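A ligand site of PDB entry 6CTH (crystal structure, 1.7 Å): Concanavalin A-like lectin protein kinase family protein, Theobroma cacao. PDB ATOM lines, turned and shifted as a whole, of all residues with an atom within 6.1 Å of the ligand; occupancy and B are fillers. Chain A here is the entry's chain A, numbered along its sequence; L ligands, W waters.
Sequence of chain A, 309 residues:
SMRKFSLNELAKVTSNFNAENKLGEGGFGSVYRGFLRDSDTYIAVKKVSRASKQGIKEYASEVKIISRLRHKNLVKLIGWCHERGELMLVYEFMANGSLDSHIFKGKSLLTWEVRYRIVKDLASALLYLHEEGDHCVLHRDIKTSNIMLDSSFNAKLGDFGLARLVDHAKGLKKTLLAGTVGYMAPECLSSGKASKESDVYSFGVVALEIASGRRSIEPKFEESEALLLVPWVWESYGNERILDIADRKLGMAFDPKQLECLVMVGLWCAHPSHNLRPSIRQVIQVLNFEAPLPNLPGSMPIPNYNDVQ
Water W1 lies within hydrogen-bond range of OH of Tyr 91 and N4 of the ligand. Water W2 lies within hydrogen-bond range of the side-chain amide oxygen (OD1) of Asn 146 (2.5 Å), the backbone NH (N) of Gly 27 (3.0 Å) and an oxygen (O3) of the ligand (3.3 Å). Water W3 bridges O of Ser 145 (2.5 Å) and O2 of the ligand (3.4 Å).
O1 of the ligand is in hydrogen-bond range of N of Met 94 (2.8 Å). The backbone carbonyl oxygen (O) of Glu 92 is in hydrogen-bond range of a nitrogen (N1) of the ligand, at 2.9 Å.
Residues that only touch the ligand: Met 148, Ala 44, Ser 98, Leu 23, Ser 145, Tyr 91, Gly 26, Phe 93, Gly 27, Asp 159, Lys 46, Gly 97, Asn 146, Gly 24, Ala 95, Val 31 and Gly 158. Hydrophobic or aromatic side chains within 4 Å of the ligand: Leu 23, Val 31, Ala 44, Tyr 91, Phe 93, Met 94 and Met 148. Of the 29 residues printed, 19 come within 4 Å of the ligand. Along chain A the residues within 4 Å of the ligand span positions 23 to 159. The nearest printed residue that does not touch the ligand is Glu 25 (4.005 Å).
The side-chain carboxylate of Asp 100 is in hydrogen-bond range of the side-chain hydroxyl of Ser 98 (2.5 Å). The backbone NH (N) of Leu 23 is in hydrogen-bond range of the backbone carbonyl oxygen (O) of Val 31. The side-chain carboxylate of Asp 159 sits close to the side-chain amide nitrogen of Asn 146, 3.0 Å away. The backbone carbonyl oxygen (O) of Gly 24 is in hydrogen-bond range of the backbone NH (N) of Val 31 (2.9 Å). The backbone carbonyl oxygen (O) of Tyr 91 lies within hydrogen-bond range of the backbone NH (N) of Ala 44. The backbone carbonyl oxygen (O) of Asn 146 is in hydrogen-bond range of the backbone NH (N) of Gly 158, at 2.9 Å.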
ATOM      1  N   GLU A  20     -12.560 -14.150  28.761  1.00  0.00           N
ATOM      2  CA  GLU A  20     -12.034 -12.819  29.036  1.00  0.00           C
ATOM      3  C   GLU A  20     -12.272 -11.892  27.830  1.00  0.00           C
ATOM      4  O   GLU A  20     -12.266 -10.672  27.988  1.00  0.00           O
ATOM      5  CB  GLU A  20     -10.546 -12.847  29.399  1.00  0.00           C
ATOM      6  CG  GLU A  20     -10.248 -13.474  30.769  1.00  0.00           C
ATOM      7  CD  GLU A  20      -8.773 -13.501  31.140  1.00  0.00           C
ATOM      8  OE1 GLU A  20      -8.352 -14.508  31.792  1.00  0.00           O
ATOM      9  OE2 GLU A  20      -8.005 -12.551  30.751  1.00  0.00           O
ATOM     10  N   LYS A  22     -15.148 -11.946  25.984  1.00  0.00           N
ATOM     11  CA  LYS A  22     -16.575 -11.773  25.765  1.00  0.00           C
ATOM     12  C   LYS A  22     -16.972 -10.309  26.020  1.00  0.00           C
ATOM     13  O   LYS A  22     -16.620  -9.736  27.070  1.00  0.00           O
ATOM     14  CB  LYS A  22     -17.395 -12.682  26.677  1.00  0.00           C
ATOM     15  N   LEU A  23     -17.641  -9.691  25.042  1.00  0.00           N
ATOM     16  CA  LEU A  23     -18.119  -8.342  25.160  1.00  0.00           C
ATOM     17  C   LEU A  23     -19.535  -8.297  25.672  1.00  0.00           C
ATOM     18  O   LEU A  23     -19.924  -7.366  26.365  1.00  0.00           O
ATOM     19  CB  LEU A  23     -18.037  -7.616  23.790  1.00  0.00           C
ATOM     20  CG  LEU A  23     -16.615  -7.364  23.292  1.00  0.00           C
ATOM     21  CD1 LEU A  23     -16.619  -6.934  21.809  1.00  0.00           C
ATOM     22  CD2 LEU A  23     -15.905  -6.330  24.167  1.00  0.00           C
ATOM     23  N   GLY A  24     -20.316  -9.321  25.344  1.00  0.00           N
ATOM     24  CA  GLY A  24     -21.728  -9.390  25.775  1.00  0.00           C
ATOM     25  C   GLY A  24     -22.471 -10.448  24.994  1.00  0.00           C
ATOM     26  O   GLY A  24     -21.912 -11.198  24.208  1.00  0.00           O
ATOM     27  N   GLU A  25     -23.763 -10.550  25.298  1.00  0.00           N
ATOM     28  CA  GLU A  25     -24.649 -11.432  24.603  1.00  0.00           C
ATOM     29  C   GLU A  25     -25.334 -10.624  23.527  1.00  0.00           C
ATOM     30  O   GLU A  25     -26.014  -9.652  23.839  1.00  0.00           O
ATOM     31  CB  GLU A  25     -25.732 -11.993  25.539  1.00  0.00           C
ATOM     32  CG  GLU A  25     -25.133 -12.852  26.651  1.00  0.00           C
ATOM     33  CD  GLU A  25     -24.258 -13.981  26.176  1.00  0.00           C
ATOM     34  OE1 GLU A  25     -24.515 -14.515  25.062  1.00  0.00           O
ATOM     35  OE2 GLU A  25     -23.312 -14.349  26.923  1.00  0.00           O
ATOM     36  N   GLY A  26     -25.191 -11.082  22.303  1.00  0.00           N
ATOM     37  CA  GLY A  26     -25.988 -10.609  21.168  1.00  0.00           C
ATOM     38  C   GLY A  26     -27.330 -11.306  21.147  1.00  0.00           C
ATOM     39  O   GLY A  26     -27.668 -12.108  22.076  1.00  0.00           O
ATOM     40  N   GLY A  27     -28.125 -11.023  20.139  1.00  0.00           N
ATOM     41  CA  GLY A  27     -29.451 -11.615  20.048  1.00  0.00           C
ATOM     42  C   GLY A  27     -29.523 -13.120  19.861  1.00  0.00           C
ATOM     43  O   GLY A  27     -30.484 -13.763  20.267  1.00  0.00           O
ATOM     44  N   PHE A  28     -28.515 -13.696  19.222  1.00  0.00           N
ATOM     45  CA  PHE A  28     -28.531 -15.123  18.883  1.00  0.00           C
ATOM     46  C   PHE A  28     -27.109 -15.684  18.936  1.00  0.00           C
ATOM     47  O   PHE A  28     -26.732 -16.590  18.157  1.00  0.00           O
ATOM     48  CB  PHE A  28     -29.257 -15.339  17.537  1.00  0.00           C
ATOM     49  CG  PHE A  28     -28.691 -14.532  16.374  1.00  0.00           C
ATOM     50  CD1 PHE A  28     -27.646 -15.041  15.594  1.00  0.00           C
ATOM     51  CD2 PHE A  28     -29.230 -13.281  16.029  1.00  0.00           C
ATOM     52  CE1 PHE A  28     -27.128 -14.310  14.516  1.00  0.00           C
ATOM     53  CE2 PHE A  28     -28.727 -12.560  14.940  1.00  0.00           C
ATOM     54  CZ  PHE A  28     -27.676 -13.075  14.183  1.00  0.00           C
ATOM     55  N   VAL A  31     -20.901 -12.289  21.744  1.00  0.00           N
ATOM     56  CA  VAL A  31     -19.981 -11.473  20.939  1.00  0.00           C
ATOM     57  C   VAL A  31     -18.636 -11.335  21.667  1.00  0.00           C
ATOM     58  O   VAL A  31     -18.599 -11.012  22.876  1.00  0.00           O
ATOM     59  CB  VAL A  31     -20.572 -10.088  20.681  1.00  0.00           C
ATOM     60  CG1 VAL A  31     -19.691  -9.263  19.736  1.00  0.00           C
ATOM     61  CG2 VAL A  31     -21.992 -10.209  20.112  1.00  0.00           C
ATOM     62  N   ALA A  44     -15.275  -7.167  16.325  1.00  0.00           N
ATOM     63  CA  ALA A  44     -16.251  -7.840  17.183  1.00  0.00           C
ATOM     64  C   ALA A  44     -16.765  -9.059  16.451  1.00  0.00           C
ATOM     65  O   ALA A  44     -17.217  -8.950  15.301  1.00  0.00           O
ATOM     66  CB  ALA A  44     -17.391  -6.899  17.524  1.00  0.00           C
ATOM     67  N   LYS A  46     -19.307 -12.256  16.500  1.00  0.00           N
ATOM     68  CA  LYS A  46     -20.460 -12.938  17.053  1.00  0.00           C
ATOM     69  C   LYS A  46     -20.440 -14.414  16.666  1.00  0.00           C
ATOM     70  O   LYS A  46     -20.452 -14.768  15.486  1.00  0.00           O
ATOM     71  CB  LYS A  46     -21.732 -12.280  16.549  1.00  0.00           C
ATOM     72  CG  LYS A  46     -22.993 -12.904  17.128  1.00  0.00           C
ATOM     73  CD  LYS A  46     -24.224 -12.056  16.867  1.00  0.00           C
ATOM     74  CE  LYS A  46     -25.423 -12.583  17.660  1.00  0.00           C
ATOM     75  NZ  LYS A  46     -26.512 -11.610  17.539  1.00  0.00           N
ATOM     76  N   VAL A  75     -25.546  -0.625  11.525  1.00  0.00           N
ATOM     77  CA  VAL A  75     -24.347  -1.401  11.681  1.00  0.00           C
ATOM     78  C   VAL A  75     -24.002  -2.136  10.387  1.00  0.00           C
ATOM     79  O   VAL A  75     -24.904  -2.689   9.749  1.00  0.00           O
ATOM     80  CB  VAL A  75     -24.560  -2.449  12.813  1.00  0.00           C
ATOM     81  CG1 VAL A  75     -23.428  -3.438  12.871  1.00  0.00           C
ATOM     82  CG2 VAL A  75     -24.749  -1.735  14.129  1.00  0.00           C
ATOM     83  N   TYR A  91     -17.974  -7.741  12.809  1.00  0.00           N
ATOM     84  CA  TYR A  91     -18.334  -6.328  12.755  1.00  0.00           C
ATOM     85  C   TYR A  91     -17.199  -5.475  13.290  1.00  0.00           C
ATOM     86  O   TYR A  91     -16.260  -6.011  13.912  1.00  0.00           O
ATOM     87  CB  TYR A  91     -19.552  -6.066  13.652  1.00  0.00           C
ATOM     88  CG  TYR A  91     -20.727  -6.989  13.493  1.00  0.00           C
ATOM     89  CD1 TYR A  91     -20.814  -8.155  14.220  1.00  0.00           C
ATOM     90  CD2 TYR A  91     -21.796  -6.633  12.671  1.00  0.00           C
ATOM     91  CE1 TYR A  91     -21.954  -8.953  14.138  1.00  0.00           C
ATOM     92  CE2 TYR A  91     -22.882  -7.444  12.554  1.00  0.00           C
ATOM     93  CZ  TYR A  91     -22.972  -8.596  13.264  1.00  0.00           C
ATOM     94  OH  TYR A  91     -24.097  -9.387  13.180  1.00  0.00           O
ATOM     95  N   GLU A  92     -17.259  -4.171  13.065  1.00  0.00           N
ATOM     96  CA  GLU A  92     -16.355  -3.236  13.746  1.00  0.00           C
ATOM     97  C   GLU A  92     -16.510  -3.294  15.245  1.00  0.00           C
ATOM     98  O   GLU A  92     -17.652  -3.438  15.759  1.00  0.00           O
ATOM     99  CB  GLU A  92     -16.553  -1.759  13.300  1.00  0.00           C
ATOM    100  N   PHE A  93     -15.373  -3.211  15.963  1.00  0.00           N
ATOM    101  CA  PHE A  93     -15.417  -3.023  17.404  1.00  0.00           C
ATOM    102  C   PHE A  93     -15.741  -1.581  17.721  1.00  0.00           C
ATOM    103  O   PHE A  93     -15.099  -0.676  17.215  1.00  0.00           O
ATOM    104  CB  PHE A  93     -14.096  -3.404  18.056  1.00  0.00           C
ATOM    105  CG  PHE A  93     -14.043  -3.094  19.501  1.00  0.00           C
ATOM    106  CD1 PHE A  93     -14.841  -3.810  20.401  1.00  0.00           C
ATOM    107  CD2 PHE A  93     -13.214  -2.079  19.983  1.00  0.00           C
ATOM    108  CE1 PHE A  93     -14.777  -3.540  21.746  1.00  0.00           C
ATOM    109  CE2 PHE A  93     -13.147  -1.822  21.346  1.00  0.00           C
ATOM    110  CZ  PHE A  93     -13.940  -2.530  22.230  1.00  0.00           C
ATOM    111  N   MET A  94     -16.747  -1.397  18.572  1.00  0.00           N
ATOM    112  CA  MET A  94     -17.254  -0.077  18.961  1.00  0.00           C
ATOM    113  C   MET A  94     -17.125   0.046  20.479  1.00  0.00           C
ATOM    114  O   MET A  94     -17.966  -0.498  21.228  1.00  0.00           O
ATOM    115  CB  MET A  94     -18.702   0.055  18.512  1.00  0.00           C
ATOM    116  CG  MET A  94     -18.845  -0.241  17.030  1.00  0.00           C
ATOM    117  SD  MET A  94     -20.494   0.021  16.315  1.00  0.00           S
ATOM    118  CE  MET A  94     -20.631   1.808  16.322  1.00  0.00           C
ATOM    119  N   ALA A  95     -16.092   0.767  20.896  1.00  0.00           N
ATOM    120  CA  ALA A  95     -15.696   0.820  22.321  1.00  0.00           C
ATOM    121  C   ALA A  95     -16.748   1.370  23.274  1.00  0.00           C
ATOM    122  O   ALA A  95     -16.760   1.070  24.463  1.00  0.00           O
ATOM    123  CB  ALA A  95     -14.395   1.628  22.433  1.00  0.00           C
ATOM    124  N   ASN A  96     -17.642   2.209  22.765  1.00  0.00           N
ATOM    125  CA  ASN A  96     -18.776   2.684  23.578  1.00  0.00           C
ATOM    126  C   ASN A  96     -19.917   1.693  23.762  1.00  0.00           C
ATOM    127  O   ASN A  96     -20.806   1.940  24.558  1.00  0.00           O
ATOM    128  CB  ASN A  96     -19.298   4.025  23.072  1.00  0.00           C
ATOM    129  CG  ASN A  96     -18.398   5.177  23.439  1.00  0.00           C
ATOM    130  OD1 ASN A  96     -17.943   5.311  24.572  1.00  0.00           O
ATOM    131  ND2 ASN A  96     -18.100   6.004  22.460  1.00  0.00           N
ATOM    132  N   GLY A  97     -19.904   0.561  23.065  1.00  0.00           N
ATOM    133  CA  GLY A  97     -20.906  -0.466  23.246  1.00  0.00           C
ATOM    134  C   GLY A  97     -22.342  -0.077  22.887  1.00  0.00           C
ATOM    135  O   GLY A  97     -22.564   0.812  22.011  1.00  0.00           O
ATOM    136  N   SER A  98     -23.311  -0.732  23.544  1.00  0.00           N
ATOM    137  CA  SER A  98     -24.699  -0.531  23.201  1.00  0.00           C
ATOM    138  C   SER A  98     -25.362   0.515  24.077  1.00  0.00           C
ATOM    139  O   SER A  98     -24.939   0.802  25.196  1.00  0.00           O
ATOM    140  CB  SER A  98     -25.488  -1.837  23.197  1.00  0.00           C
ATOM    141  OG  SER A  98     -25.281  -2.586  24.389  1.00  0.00           O
ATOM    142  N   ASP A 100     -28.163   0.728  25.755  1.00  0.00           N
ATOM    143  CA  ASP A 100     -28.710   0.266  27.044  1.00  0.00           C
ATOM    144  C   ASP A 100     -27.686   0.411  28.202  1.00  0.00           C
ATOM    145  O   ASP A 100     -28.060   0.772  29.304  1.00  0.00           O
ATOM    146  CB  ASP A 100     -29.254  -1.175  26.942  1.00  0.00           C
ATOM    147  CG  ASP A 100     -28.194  -2.188  26.571  1.00  0.00           C
ATOM    148  OD1 ASP A 100     -27.358  -1.926  25.650  1.00  0.00           O
ATOM    149  OD2 ASP A 100     -28.142  -3.275  27.224  1.00  0.00           O
ATOM    150  N   SER A 101     -26.407   0.185  27.913  1.00  0.00           N
ATOM    151  CA  SER A 101     -25.323   0.261  28.904  1.00  0.00           C
ATOM    152  C   SER A 101     -25.152   1.651  29.423  1.00  0.00           C
ATOM    153  O   SER A 101     -24.803   1.825  30.586  1.00  0.00           O
ATOM    154  CB  SER A 101     -24.020  -0.231  28.345  1.00  0.00           C
ATOM    155  OG  SER A 101     -24.144  -1.612  28.085  1.00  0.00           O
ATOM    156  N   SER A 145     -30.652  -2.165  23.403  1.00  0.00           N
ATOM    157  CA  SER A 145     -29.534  -3.083  23.291  1.00  0.00           C
ATOM    158  C   SER A 145     -29.108  -3.426  21.862  1.00  0.00           C
ATOM    159  O   SER A 145     -28.077  -4.070  21.669  1.00  0.00           O
ATOM    160  CB  SER A 145     -29.773  -4.406  24.047  1.00  0.00           C
ATOM    161  OG  SER A 145     -30.966  -5.045  23.614  1.00  0.00           O
ATOM    162  N   ASN A 146     -29.940  -3.058  20.884  1.00  0.00           N
ATOM    163  CA  ASN A 146     -29.603  -3.194  19.494  1.00  0.00           C
ATOM    164  C   ASN A 146     -29.116  -1.914  18.865  1.00  0.00           C
ATOM    165  O   ASN A 146     -28.913  -1.891  17.614  1.00  0.00           O
ATOM    166  CB  ASN A 146     -30.794  -3.724  18.692  1.00  0.00           C
ATOM    167  CG  ASN A 146     -31.017  -5.206  18.911  1.00  0.00           C
ATOM    168  OD1 ASN A 146     -30.082  -5.953  19.258  1.00  0.00           O
ATOM    169  ND2 ASN A 146     -32.217  -5.639  18.712  1.00  0.00           N
ATOM    170  N   ILE A 147     -28.885  -0.881  19.659  1.00  0.00           N
ATOM    171  CA  ILE A 147     -28.324   0.389  19.147  1.00  0.00           C
ATOM    172  C   ILE A 147     -26.885   0.558  19.652  1.00  0.00           C
ATOM    173  O   ILE A 147     -26.638   0.649  20.854  1.00  0.00           O
ATOM    174  CB  ILE A 147     -29.215   1.584  19.556  1.00  0.00           C
ATOM    175  CG1 ILE A 147     -30.629   1.371  19.024  1.00  0.00           C
ATOM    176  CG2 ILE A 147     -28.623   2.899  19.089  1.00  0.00           C
ATOM    177  CD1 ILE A 147     -31.658   2.363  19.538  1.00  0.00           C
ATOM    178  N   MET A 148     -25.942   0.603  18.695  1.00  0.00           N
ATOM    179  CA  MET A 148     -24.532   0.745  19.011  1.00  0.00           C
ATOM    180  C   MET A 148     -24.126   2.193  18.947  1.00  0.00           C
ATOM    181  O   MET A 148     -24.702   2.979  18.136  1.00  0.00           O
ATOM    182  CB  MET A 148     -23.686  -0.058  18.019  1.00  0.00           C
ATOM    183  CG  MET A 148     -23.938  -1.548  18.022  1.00  0.00           C
ATOM    184  SD  MET A 148     -23.660  -2.270  19.679  1.00  0.00           S
ATOM    185  CE  MET A 148     -21.932  -1.904  19.777  1.00  0.00           C
ATOM    186  N   LEU A 157     -28.125   1.284  14.358  1.00  0.00           N
ATOM    187  CA  LEU A 157     -29.046   0.215  14.642  1.00  0.00           C
ATOM    188  C   LEU A 157     -28.525  -1.057  14.023  1.00  0.00           C
ATOM    189  O   LEU A 157     -28.030  -1.079  12.892  1.00  0.00           O
ATOM    190  CB  LEU A 157     -30.426   0.576  14.135  1.00  0.00           C
ATOM    191  CG  LEU A 157     -31.480  -0.487  14.196  1.00  0.00           C
ATOM    192  CD1 LEU A 157     -31.852  -0.778  15.649  1.00  0.00           C
ATOM    193  CD2 LEU A 157     -32.730  -0.052  13.456  1.00  0.00           C
ATOM    194  N   GLY A 158     -28.550  -2.141  14.780  1.00  0.00           N
ATOM    195  CA  GLY A 158     -28.191  -3.440  14.289  1.00  0.00           C
ATOM    196  C   GLY A 158     -29.170  -4.512  14.692  1.00  0.00           C
ATOM    197  O   GLY A 158     -30.267  -4.209  15.145  1.00  0.00           O
ATOM    198  N   ASP A 159     -28.683  -5.745  14.625  1.00  0.00           N
ATOM    199  CA  ASP A 159     -29.447  -6.985  14.830  1.00  0.00           C
ATOM    200  C   ASP A 159     -30.590  -7.170  13.868  1.00  0.00           C
ATOM    201  O   ASP A 159     -31.754  -6.828  14.175  1.00  0.00           O
ATOM    202  CB  ASP A 159     -30.040  -7.048  16.284  1.00  0.00           C
ATOM    203  CG  ASP A 159     -30.783  -8.363  16.566  1.00  0.00           C
ATOM    204  OD1 ASP A 159     -30.531  -9.378  15.898  1.00  0.00           O
ATOM    205  OD2 ASP A 159     -31.655  -8.303  17.473  1.00  0.00           O
HETATM  206  C1  LIG L   1     -21.260  -5.306  18.944  1.00  0.00           C
HETATM  207  C2  LIG L   1     -23.495  -6.563  23.453  1.00  0.00           C
HETATM  208  C3  LIG L   1     -20.729  -5.044  17.676  1.00  0.00           C
HETATM  209  C4  LIG L   1     -21.391  -5.428  16.515  1.00  0.00           C
HETATM  210  C5  LIG L   1     -21.392  -5.357  22.086  1.00  0.00           C
HETATM  211  C6  LIG L   1     -22.613  -6.064  16.628  1.00  0.00           C
HETATM  212  C7  LIG L   1     -19.221  -4.172  19.113  1.00  0.00           C
HETATM  213  C8  LIG L   1     -20.311  -4.772  19.920  1.00  0.00           C
HETATM  214  C9  LIG L   1     -20.329  -4.720  21.300  1.00  0.00           C
HETATM  215  C10 LIG L   1     -21.523  -6.739  22.119  1.00  0.00           C
HETATM  216  C11 LIG L   1     -22.567  -7.342  22.787  1.00  0.00           C
HETATM  217  N1  LIG L   1     -19.531  -4.362  17.814  1.00  0.00           N
HETATM  218  N2  LIG L   1     -19.385  -3.984  21.906  1.00  0.00           N
HETATM  219  C12 LIG L   1     -22.509  -5.931  19.041  1.00  0.00           C
HETATM  220  N3  LIG L   1     -16.815  -3.689  27.797  1.00  0.00           N
HETATM  221  O1  LIG L   1     -18.222  -3.605  19.533  1.00  0.00           O
HETATM  222  C13 LIG L   1     -23.193  -6.272  17.870  1.00  0.00           C
HETATM  223  N4  LIG L   1     -24.522  -6.780  17.904  1.00  0.00           N
HETATM  224  S1  LIG L   1     -25.513  -7.062  19.148  1.00  0.00           S
HETATM  225  O2  LIG L   1     -24.736  -7.169  20.346  1.00  0.00           O
HETATM  226  O3  LIG L   1     -26.370  -8.134  18.768  1.00  0.00           O
HETATM  227  C14 LIG L   1     -26.392  -5.535  19.117  1.00  0.00           C
HETATM  228  C15 LIG L   1     -26.722  -5.222  17.680  1.00  0.00           C
HETATM  229  C16 LIG L   1     -22.329  -4.594  22.764  1.00  0.00           C
HETATM  230  C17 LIG L   1     -23.373  -5.193  23.446  1.00  0.00           C
HETATM  231  C18 LIG L   1     -19.039  -3.757  23.261  1.00  0.00           C
HETATM  232  C19 LIG L   1     -19.684  -4.411  24.308  1.00  0.00           C
HETATM  233  C20 LIG L   1     -19.336  -4.125  25.612  1.00  0.00           C
HETATM  234  C21 LIG L   1     -18.352  -3.195  25.906  1.00  0.00           C
HETATM  235  C22 LIG L   1     -17.723  -2.548  24.861  1.00  0.00           C
HETATM  236  C23 LIG L   1     -18.056  -2.830  23.541  1.00  0.00           C
HETATM  237  C24 LIG L   1     -17.965  -2.896  27.337  1.00  0.00           C
HETATM  238  C25 LIG L   1     -16.384  -3.258  29.135  1.00  0.00           C
HETATM  239  C26 LIG L   1     -15.151  -4.001  29.581  1.00  0.00           C
HETATM  240  C27 LIG L   1     -15.370  -5.499  29.556  1.00  0.00           C
HETATM  241  C28 LIG L   1     -15.932  -5.940  28.225  1.00  0.00           C
HETATM  242  C29 LIG L   1     -17.139  -5.112  27.845  1.00  0.00           C
HETATM  243  O   HOH W   1     -25.437  -8.658  15.597  1.00  0.00           O
HETATM  244  O   HOH W   2     -29.479  -8.302  19.959  1.00  0.00           O
HETATM  245  O   HOH W   3     -26.724  -5.869  22.809  1.00  0.00           O
